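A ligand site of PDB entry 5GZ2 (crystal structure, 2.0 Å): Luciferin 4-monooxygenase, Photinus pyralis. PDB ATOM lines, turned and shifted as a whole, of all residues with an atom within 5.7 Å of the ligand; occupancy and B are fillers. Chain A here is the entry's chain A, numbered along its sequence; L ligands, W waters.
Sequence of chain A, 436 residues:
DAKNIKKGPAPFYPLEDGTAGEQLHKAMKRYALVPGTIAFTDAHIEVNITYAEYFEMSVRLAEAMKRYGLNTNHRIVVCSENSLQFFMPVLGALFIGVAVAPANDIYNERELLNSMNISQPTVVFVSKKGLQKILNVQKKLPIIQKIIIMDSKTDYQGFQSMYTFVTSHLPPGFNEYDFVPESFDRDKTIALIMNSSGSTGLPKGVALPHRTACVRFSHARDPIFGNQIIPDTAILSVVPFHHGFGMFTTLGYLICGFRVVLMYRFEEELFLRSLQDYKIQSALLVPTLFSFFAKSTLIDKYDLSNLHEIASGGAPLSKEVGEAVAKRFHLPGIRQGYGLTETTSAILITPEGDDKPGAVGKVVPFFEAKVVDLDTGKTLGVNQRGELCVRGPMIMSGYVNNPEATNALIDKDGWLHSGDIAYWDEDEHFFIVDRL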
ATOM      1  N   ARG A 216      26.721 -19.428 -13.002  1.00  0.00           N
ATOM      2  CA  ARG A 216      25.787 -18.868 -12.029  1.00  0.00           C
ATOM      3  C   ARG A 216      24.929 -19.959 -11.380  1.00  0.00           C
ATOM      4  O   ARG A 216      24.645 -19.900 -10.184  1.00  0.00           O
ATOM      5  CB  ARG A 216      24.897 -17.822 -12.683  1.00  0.00           C
ATOM      6  CG  ARG A 216      23.764 -17.336 -11.777  1.00  0.00           C
ATOM      7  CD  ARG A 216      24.263 -16.752 -10.453  1.00  0.00           C
ATOM      8  NE  ARG A 216      23.188 -16.715  -9.472  1.00  0.00           N
ATOM      9  CZ  ARG A 216      23.330 -16.430  -8.184  1.00  0.00           C
ATOM     10  NH1 ARG A 216      24.528 -16.137  -7.666  1.00  0.00           N
ATOM     11  NH2 ARG A 216      22.267 -16.442  -7.385  1.00  0.00           N
ATOM     12  N   PHE A 225      27.658 -20.696  -1.170  1.00  0.00           N
ATOM     13  CA  PHE A 225      27.569 -19.485  -1.977  1.00  0.00           C
ATOM     14  C   PHE A 225      26.191 -19.256  -2.570  1.00  0.00           C
ATOM     15  O   PHE A 225      26.005 -18.308  -3.333  1.00  0.00           O
ATOM     16  CB  PHE A 225      28.611 -19.524  -3.091  1.00  0.00           C
ATOM     17  CG  PHE A 225      30.002 -19.333  -2.582  1.00  0.00           C
ATOM     18  CD1 PHE A 225      30.789 -20.419  -2.243  1.00  0.00           C
ATOM     19  CD2 PHE A 225      30.514 -18.056  -2.390  1.00  0.00           C
ATOM     20  CE1 PHE A 225      32.068 -20.244  -1.757  1.00  0.00           C
ATOM     21  CE2 PHE A 225      31.790 -17.872  -1.908  1.00  0.00           C
ATOM     22  CZ  PHE A 225      32.564 -18.964  -1.598  1.00  0.00           C
ATOM     23  N   GLY A 226      25.223 -20.114  -2.251  1.00  0.00           N
ATOM     24  CA  GLY A 226      23.890 -19.959  -2.792  1.00  0.00           C
ATOM     25  C   GLY A 226      22.877 -20.334  -1.734  1.00  0.00           C
ATOM     26  O   GLY A 226      23.024 -19.959  -0.574  1.00  0.00           O
ATOM     27  N   GLY A 244      20.703  -7.587 -13.860  1.00  0.00           N
ATOM     28  CA  GLY A 244      21.415  -8.828 -13.609  1.00  0.00           C
ATOM     29  C   GLY A 244      21.138  -9.413 -12.240  1.00  0.00           C
ATOM     30  O   GLY A 244      21.094 -10.638 -12.070  1.00  0.00           O
ATOM     31  N   PHE A 245      20.926  -8.547 -11.255  1.00  0.00           N
ATOM     32  CA  PHE A 245      20.587  -8.998  -9.919  1.00  0.00           C
ATOM     33  C   PHE A 245      19.320  -9.844  -9.939  1.00  0.00           C
ATOM     34  O   PHE A 245      19.314 -10.995  -9.498  1.00  0.00           O
ATOM     35  CB  PHE A 245      20.475  -7.762  -9.007  1.00  0.00           C
ATOM     36  CG  PHE A 245      20.245  -8.075  -7.548  1.00  0.00           C
ATOM     37  CD1 PHE A 245      20.550  -9.311  -7.009  1.00  0.00           C
ATOM     38  CD2 PHE A 245      19.717  -7.095  -6.700  1.00  0.00           C
ATOM     39  CE1 PHE A 245      20.320  -9.577  -5.663  1.00  0.00           C
ATOM     40  CE2 PHE A 245      19.489  -7.356  -5.346  1.00  0.00           C
ATOM     41  CZ  PHE A 245      19.793  -8.592  -4.831  1.00  0.00           C
ATOM     42  N   THR A 249      19.479 -14.203 -10.076  1.00  0.00           N
ATOM     43  CA  THR A 249      18.908 -14.877  -8.926  1.00  0.00           C
ATOM     44  C   THR A 249      17.669 -15.680  -9.346  1.00  0.00           C
ATOM     45  O   THR A 249      17.508 -16.831  -8.959  1.00  0.00           O
ATOM     46  CB  THR A 249      18.539 -13.897  -7.806  1.00  0.00           C
ATOM     47  OG1 THR A 249      17.585 -12.926  -8.261  1.00  0.00           O
ATOM     48  CG2 THR A 249      19.783 -13.183  -7.239  1.00  0.00           C
ATOM     49  N   LEU A 284      14.785 -10.438  -0.956  1.00  0.00           N
ATOM     50  CA  LEU A 284      15.678  -9.778  -1.908  1.00  0.00           C
ATOM     51  C   LEU A 284      15.281  -8.328  -2.067  1.00  0.00           C
ATOM     52  O   LEU A 284      14.175  -8.016  -2.513  1.00  0.00           O
ATOM     53  CB  LEU A 284      15.630 -10.503  -3.249  1.00  0.00           C
ATOM     54  CG  LEU A 284      16.573 -11.680  -3.349  1.00  0.00           C
ATOM     55  CD1 LEU A 284      17.971 -11.154  -3.503  1.00  0.00           C
ATOM     56  CD2 LEU A 284      16.493 -12.624  -2.178  1.00  0.00           C
ATOM     57  N   GLU A 309      17.125 -14.991   6.025  1.00  0.00           N
ATOM     58  CA  GLU A 309      18.108 -14.048   5.530  1.00  0.00           C
ATOM     59  C   GLU A 309      17.423 -12.928   4.770  1.00  0.00           C
ATOM     60  O   GLU A 309      16.366 -13.116   4.152  1.00  0.00           O
ATOM     61  CB  GLU A 309      19.144 -14.731   4.629  1.00  0.00           C
ATOM     62  CG  GLU A 309      18.682 -14.828   3.186  1.00  0.00           C
ATOM     63  CD  GLU A 309      19.645 -15.611   2.297  1.00  0.00           C
ATOM     64  OE1 GLU A 309      20.769 -15.906   2.764  1.00  0.00           O
ATOM     65  OE2 GLU A 309      19.269 -15.904   1.134  1.00  0.00           O
ATOM     66  N   ALA A 311      18.772 -10.506   1.773  1.00  0.00           N
ATOM     67  CA  ALA A 311      19.897 -10.434   0.855  1.00  0.00           C
ATOM     68  C   ALA A 311      19.944  -9.061   0.195  1.00  0.00           C
ATOM     69  O   ALA A 311      18.917  -8.412  -0.018  1.00  0.00           O
ATOM     70  CB  ALA A 311      19.819 -11.521  -0.224  1.00  0.00           C
ATOM     71  N   SER A 312      21.148  -8.649  -0.150  1.00  0.00           N
ATOM     72  CA  SER A 312      21.384  -7.340  -0.694  1.00  0.00           C
ATOM     73  C   SER A 312      22.349  -7.449  -1.861  1.00  0.00           C
ATOM     74  O   SER A 312      23.262  -8.271  -1.845  1.00  0.00           O
ATOM     75  CB  SER A 312      21.989  -6.398   0.357  1.00  0.00           C
ATOM     76  OG  SER A 312      21.911  -5.050  -0.086  1.00  0.00           O
ATOM     77  N   GLY A 313      22.157  -6.597  -2.844  1.00  0.00           N
ATOM     78  CA  GLY A 313      23.209  -6.487  -3.843  1.00  0.00           C
ATOM     79  C   GLY A 313      23.011  -5.280  -4.706  1.00  0.00           C
ATOM     80  O   GLY A 313      22.058  -4.512  -4.555  1.00  0.00           O
ATOM     81  N   GLY A 314      23.976  -5.102  -5.618  1.00  0.00           N
ATOM     82  CA  GLY A 314      23.836  -4.223  -6.757  1.00  0.00           C
ATOM     83  C   GLY A 314      24.208  -2.767  -6.549  1.00  0.00           C
ATOM     84  O   GLY A 314      24.179  -2.003  -7.526  1.00  0.00           O
ATOM     85  N   ALA A 315      24.561  -2.353  -5.327  1.00  0.00           N
ATOM     86  CA  ALA A 315      24.757  -0.927  -5.051  1.00  0.00           C
ATOM     87  C   ALA A 315      25.350  -0.784  -3.645  1.00  0.00           C
ATOM     88  O   ALA A 315      25.672  -1.804  -3.034  1.00  0.00           O
ATOM     89  CB  ALA A 315      23.415  -0.198  -5.235  1.00  0.00           C
ATOM     90  N   ARG A 335      22.977 -10.481   4.344  1.00  0.00           N
ATOM     91  CA  ARG A 335      23.701 -11.325   3.406  1.00  0.00           C
ATOM     92  C   ARG A 335      23.851 -10.587   2.089  1.00  0.00           C
ATOM     93  O   ARG A 335      22.855 -10.250   1.442  1.00  0.00           O
ATOM     94  CB  ARG A 335      23.027 -12.676   3.219  1.00  0.00           C
ATOM     95  CG  ARG A 335      23.835 -13.562   2.313  1.00  0.00           C
ATOM     96  CD  ARG A 335      23.943 -14.971   2.854  1.00  0.00           C
ATOM     97  NE  ARG A 335      24.687 -15.811   1.932  1.00  0.00           N
ATOM     98  CZ  ARG A 335      24.186 -16.889   1.338  1.00  0.00           C
ATOM     99  NH1 ARG A 335      22.935 -17.257   1.589  1.00  0.00           N
ATOM    100  NH2 ARG A 335      24.938 -17.593   0.503  1.00  0.00           N
ATOM    101  N   GLN A 336      25.088 -10.339   1.683  1.00  0.00           N
ATOM    102  CA  GLN A 336      25.358  -9.349   0.661  1.00  0.00           C
ATOM    103  C   GLN A 336      26.177  -9.979  -0.462  1.00  0.00           C
ATOM    104  O   GLN A 336      26.705 -11.082  -0.325  1.00  0.00           O
ATOM    105  CB  GLN A 336      26.091  -8.156   1.273  1.00  0.00           C
ATOM    106  CG  GLN A 336      25.881  -6.835   0.577  1.00  0.00           C
ATOM    107  CD  GLN A 336      26.674  -5.736   1.237  1.00  0.00           C
ATOM    108  OE1 GLN A 336      27.204  -5.906   2.340  1.00  0.00           O
ATOM    109  NE2 GLN A 336      26.784  -4.602   0.561  1.00  0.00           N
ATOM    110  N   GLY A 337      26.299  -9.244  -1.561  1.00  0.00           N
ATOM    111  CA  GLY A 337      27.092  -9.706  -2.676  1.00  0.00           C
ATOM    112  C   GLY A 337      27.388  -8.589  -3.650  1.00  0.00           C
ATOM    113  O   GLY A 337      26.668  -7.578  -3.713  1.00  0.00           O
ATOM    114  N   TYR A 338      28.446  -8.782  -4.424  1.00  0.00           N
ATOM    115  CA  TYR A 338      28.901  -7.737  -5.326  1.00  0.00           C
ATOM    116  C   TYR A 338      29.158  -8.303  -6.711  1.00  0.00           C
ATOM    117  O   TYR A 338      29.834  -9.328  -6.856  1.00  0.00           O
ATOM    118  CB  TYR A 338      30.169  -7.067  -4.777  1.00  0.00           C
ATOM    119  CG  TYR A 338      30.861  -6.172  -5.761  1.00  0.00           C
ATOM    120  CD1 TYR A 338      31.857  -6.675  -6.584  1.00  0.00           C
ATOM    121  CD2 TYR A 338      30.547  -4.834  -5.858  1.00  0.00           C
ATOM    122  CE1 TYR A 338      32.495  -5.883  -7.474  1.00  0.00           C
ATOM    123  CE2 TYR A 338      31.197  -4.016  -6.756  1.00  0.00           C
ATOM    124  CZ  TYR A 338      32.167  -4.558  -7.559  1.00  0.00           C
ATOM    125  OH  TYR A 338      32.834  -3.787  -8.472  1.00  0.00           O
ATOM    126  N   GLY A 339      28.625  -7.611  -7.722  1.00  0.00           N
ATOM    127  CA  GLY A 339      28.956  -7.885  -9.112  1.00  0.00           C
ATOM    128  C   GLY A 339      28.549  -6.716  -9.976  1.00  0.00           C
ATOM    129  O   GLY A 339      27.937  -5.747  -9.505  1.00  0.00           O
ATOM    130  N   LEU A 340      28.890  -6.809 -11.258  1.00  0.00           N
ATOM    131  CA  LEU A 340      28.512  -5.807 -12.239  1.00  0.00           C
ATOM    132  C   LEU A 340      27.694  -6.474 -13.327  1.00  0.00           C
ATOM    133  O   LEU A 340      27.688  -7.695 -13.465  1.00  0.00           O
ATOM    134  CB  LEU A 340      29.732  -5.135 -12.854  1.00  0.00           C
ATOM    135  CG  LEU A 340      30.756  -4.549 -11.876  1.00  0.00           C
ATOM    136  CD1 LEU A 340      31.922  -3.951 -12.658  1.00  0.00           C
ATOM    137  CD2 LEU A 340      30.082  -3.517 -10.995  1.00  0.00           C
ATOM    138  N   THR A 341      26.998  -5.659 -14.122  1.00  0.00           N
ATOM    139  CA  THR A 341      26.318  -6.194 -15.301  1.00  0.00           C
ATOM    140  C   THR A 341      27.312  -6.966 -16.170  1.00  0.00           C
ATOM    141  O   THR A 341      26.987  -8.068 -16.654  1.00  0.00           O
ATOM    142  CB  THR A 341      25.661  -5.062 -16.089  1.00  0.00           C
ATOM    143  OG1 THR A 341      24.733  -4.380 -15.226  1.00  0.00           O
ATOM    144  CG2 THR A 341      24.926  -5.608 -17.316  1.00  0.00           C
ATOM    145  N   THR A 344      28.033 -10.802 -15.139  1.00  0.00           N
ATOM    146  CA  THR A 344      26.884 -11.664 -15.022  1.00  0.00           C
ATOM    147  C   THR A 344      26.146 -11.484 -13.711  1.00  0.00           C
ATOM    148  O   THR A 344      25.073 -10.957 -13.689  1.00  0.00           O
ATOM    149  CB  THR A 344      27.293 -13.129 -15.187  1.00  0.00           C
ATOM    150  OG1 THR A 344      27.618 -13.356 -16.543  1.00  0.00           O
ATOM    151  CG2 THR A 344      26.214 -14.010 -14.828  1.00  0.00           C
ATOM    152  N   SER A 345      26.753 -11.911 -12.628  1.00  0.00           N
ATOM    153  CA  SER A 345      26.105 -11.974 -11.351  1.00  0.00           C
ATOM    154  C   SER A 345      27.098 -11.607 -10.269  1.00  0.00           C
ATOM    155  O   SER A 345      28.060 -10.960 -10.521  1.00  0.00           O
ATOM    156  CB  SER A 345      25.622 -13.388 -11.144  1.00  0.00           C
ATOM    157  OG  SER A 345      24.878 -13.486  -9.982  1.00  0.00           O
ATOM    158  N   ALA A 346      26.866 -12.050  -9.061  1.00  0.00           N
ATOM    159  CA  ALA A 346      27.755 -11.701  -7.991  1.00  0.00           C
ATOM    160  C   ALA A 346      29.055 -12.490  -7.987  1.00  0.00           C
ATOM    161  O   ALA A 346      29.061 -13.684  -8.158  1.00  0.00           O
ATOM    162  CB  ALA A 346      27.057 -11.792  -6.667  1.00  0.00           C
ATOM    163  N   ILE A 349      30.447 -12.790  -2.556  1.00  0.00           N
ATOM    164  CA  ILE A 349      29.204 -13.238  -1.920  1.00  0.00           C
ATOM    165  C   ILE A 349      29.473 -13.580  -0.464  1.00  0.00           C
ATOM    166  O   ILE A 349      30.395 -14.339  -0.173  1.00  0.00           O
ATOM    167  CB  ILE A 349      28.642 -14.470  -2.643  1.00  0.00           C
ATOM    168  CG1 ILE A 349      28.151 -14.090  -4.043  1.00  0.00           C
ATOM    169  CG2 ILE A 349      27.587 -15.125  -1.782  1.00  0.00           C
ATOM    170  CD1 ILE A 349      27.513 -15.212  -4.816  1.00  0.00           C
ATOM    171  N   THR A 350      28.655 -13.031   0.438  1.00  0.00           N
ATOM    172  CA  THR A 350      28.640 -13.488   1.821  1.00  0.00           C
ATOM    173  C   THR A 350      28.390 -15.002   1.871  1.00  0.00           C
ATOM    174  O   THR A 350      27.322 -15.458   1.440  1.00  0.00           O
ATOM    175  CB  THR A 350      27.576 -12.758   2.643  1.00  0.00           C
ATOM    176  OG1 THR A 350      27.804 -11.336   2.594  1.00  0.00           O
ATOM    177  CG2 THR A 350      27.638 -13.196   4.096  1.00  0.00           C
HETATM  178  O1  LIG L   1      25.621  -3.995 -11.273  1.00  0.00           O
HETATM  179  C1  LIG L   1      25.183  -4.450 -10.227  1.00  0.00           C
HETATM  180  O2  LIG L   1      25.121  -3.816  -9.171  1.00  0.00           O
HETATM  181  C2  LIG L   1      24.581  -5.705 -10.267  1.00  0.00           C
HETATM  182  N1  LIG L   1      24.601  -6.448  -8.982  1.00  0.00           N
HETATM  183  C3  LIG L   1      25.171  -6.635 -11.287  1.00  0.00           C
HETATM  184  S1  LIG L   1      24.561  -8.158 -10.702  1.00  0.00           S
HETATM  185  C4  LIG L   1      24.602  -7.762  -9.152  1.00  0.00           C
HETATM  186  C5  LIG L   1      24.399  -8.668  -8.228  1.00  0.00           C
HETATM  187  N2  LIG L   1      23.973  -9.818  -8.573  1.00  0.00           N
HETATM  188  S2  LIG L   1      24.459  -8.602  -6.780  1.00  0.00           S
HETATM  189  C6  LIG L   1      24.048  -9.925  -6.385  1.00  0.00           C
HETATM  190  C7  LIG L   1      23.907 -10.530  -5.211  1.00  0.00           C
HETATM  191  C8  LIG L   1      23.790 -10.542  -7.520  1.00  0.00           C
HETATM  192  C9  LIG L   1      23.389 -11.761  -7.530  1.00  0.00           C
HETATM  193  C10 LIG L   1      23.217 -12.459  -6.375  1.00  0.00           C
HETATM  194  C11 LIG L   1      23.468 -11.847  -5.186  1.00  0.00           C
HETATM  195  N3  LIG L   1      23.293 -12.620  -4.118  1.00  0.00           N
HETATM  196  C12 LIG L   1      23.818 -13.982  -4.252  1.00  0.00           C
HETATM  197  C13 LIG L   1      24.489 -14.455  -3.044  1.00  0.00           C
HETATM  198  C14 LIG L   1      23.549 -14.578  -1.919  1.00  0.00           C
HETATM  199  C15 LIG L   1      23.645 -13.348  -1.053  1.00  0.00           C
HETATM  200  C16 LIG L   1      23.491 -12.023  -1.771  1.00  0.00           C
HETATM  201  C17 LIG L   1      22.606 -12.094  -2.969  1.00  0.00           C
HETATM  202  O   HOH W   1      26.552  -5.724  -6.666  1.00  0.00           O
HETATM  203  O   HOH W   2      24.404 -17.148  -5.272  1.00  0.00           O
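N of Phe 245 lies close to S1 of the ligand (3.7 Å).
An oxygen (O2) of the ligand lies close to the backbone carbonyl oxygen (O) of Gly 314, at 2.6 Å.
S2 of the ligand sits close to N of Gly 314 (3.7 Å).
Water W1 lies within hydrogen-bond range of the backbone NH (N) of Gly 314 (2.8 Å), the backbone NH (N) of Gly 339 (3.0 Å), a nitrogen (N1) of the ligand (3.1 Å) and the backbone carbonyl oxygen (O) of Gly 337 (3.5 Å).
Water W2 bridges the guanidinium group of Arg 216 (2.6 Å) and the backbone carbonyl oxygen of Phe 225 (2.8 Å).
The backbone carbonyl oxygen (O) of Gly 339 sits close to an oxygen (O1) of the ligand.
C of Gly 244 touches S1 of the ligand (3.96 Å).
Thr 249 touches the ligand (CG2 to C10, 3.6 Å).
CB of Ala 311 touches C17 of the ligand, 3.95 Å away.
Ser 312 touches the ligand (O to C16, 3.8 Å).
CA of Gly 313 touches S2 of the ligand, at 3.8 Å.
CG of Arg 335 touches C15 of the ligand (3.4 Å).
Gln 336 touches the ligand.
Gly 337 touches the ligand.
Leu 340 touches the ligand.
Thr 341 touches the ligand.
Ser 345 touches the ligand.
CB of Ala 346 touches C6 of the ligand (3.6 Å).
Ile 349 touches the ligand (CG2 to C13, 3.4 Å).
Hydrophobic or aromatic side chains that line the ligand: Phe 245, Ala 311, Ala 346 and Ile 349.
NH1 of Arg 335 lies within salt-bridge range of OE1 of Glu 309 (2.8 Å).
The backbone carbonyl oxygen (O) of Arg 335 is in hydrogen-bond range of the backbone NH (N) of Ser 312, 2.8 Å away.
O of Ser 312 is in hydrogen-bond range of N of Gly 337 (3.2 Å).
O of Gly 226 is in hydrogen-bond range of NH2 of Arg 335 (3.2 Å).
The backbone carbonyl oxygen of Thr 350 lies within hydrogen-bond range of the guanidinium group of Arg 335, at 2.7 Å.
The side-chain hydroxyl (OG1) of Thr 249 sits at hydrogen-bond distance from the backbone carbonyl oxygen (O) of Phe 245 (2.9 Å).
The backbone NH (N) of Thr 350 is in hydrogen-bond range of the backbone carbonyl oxygen (O) of Gln 336, 2.9 Å away.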
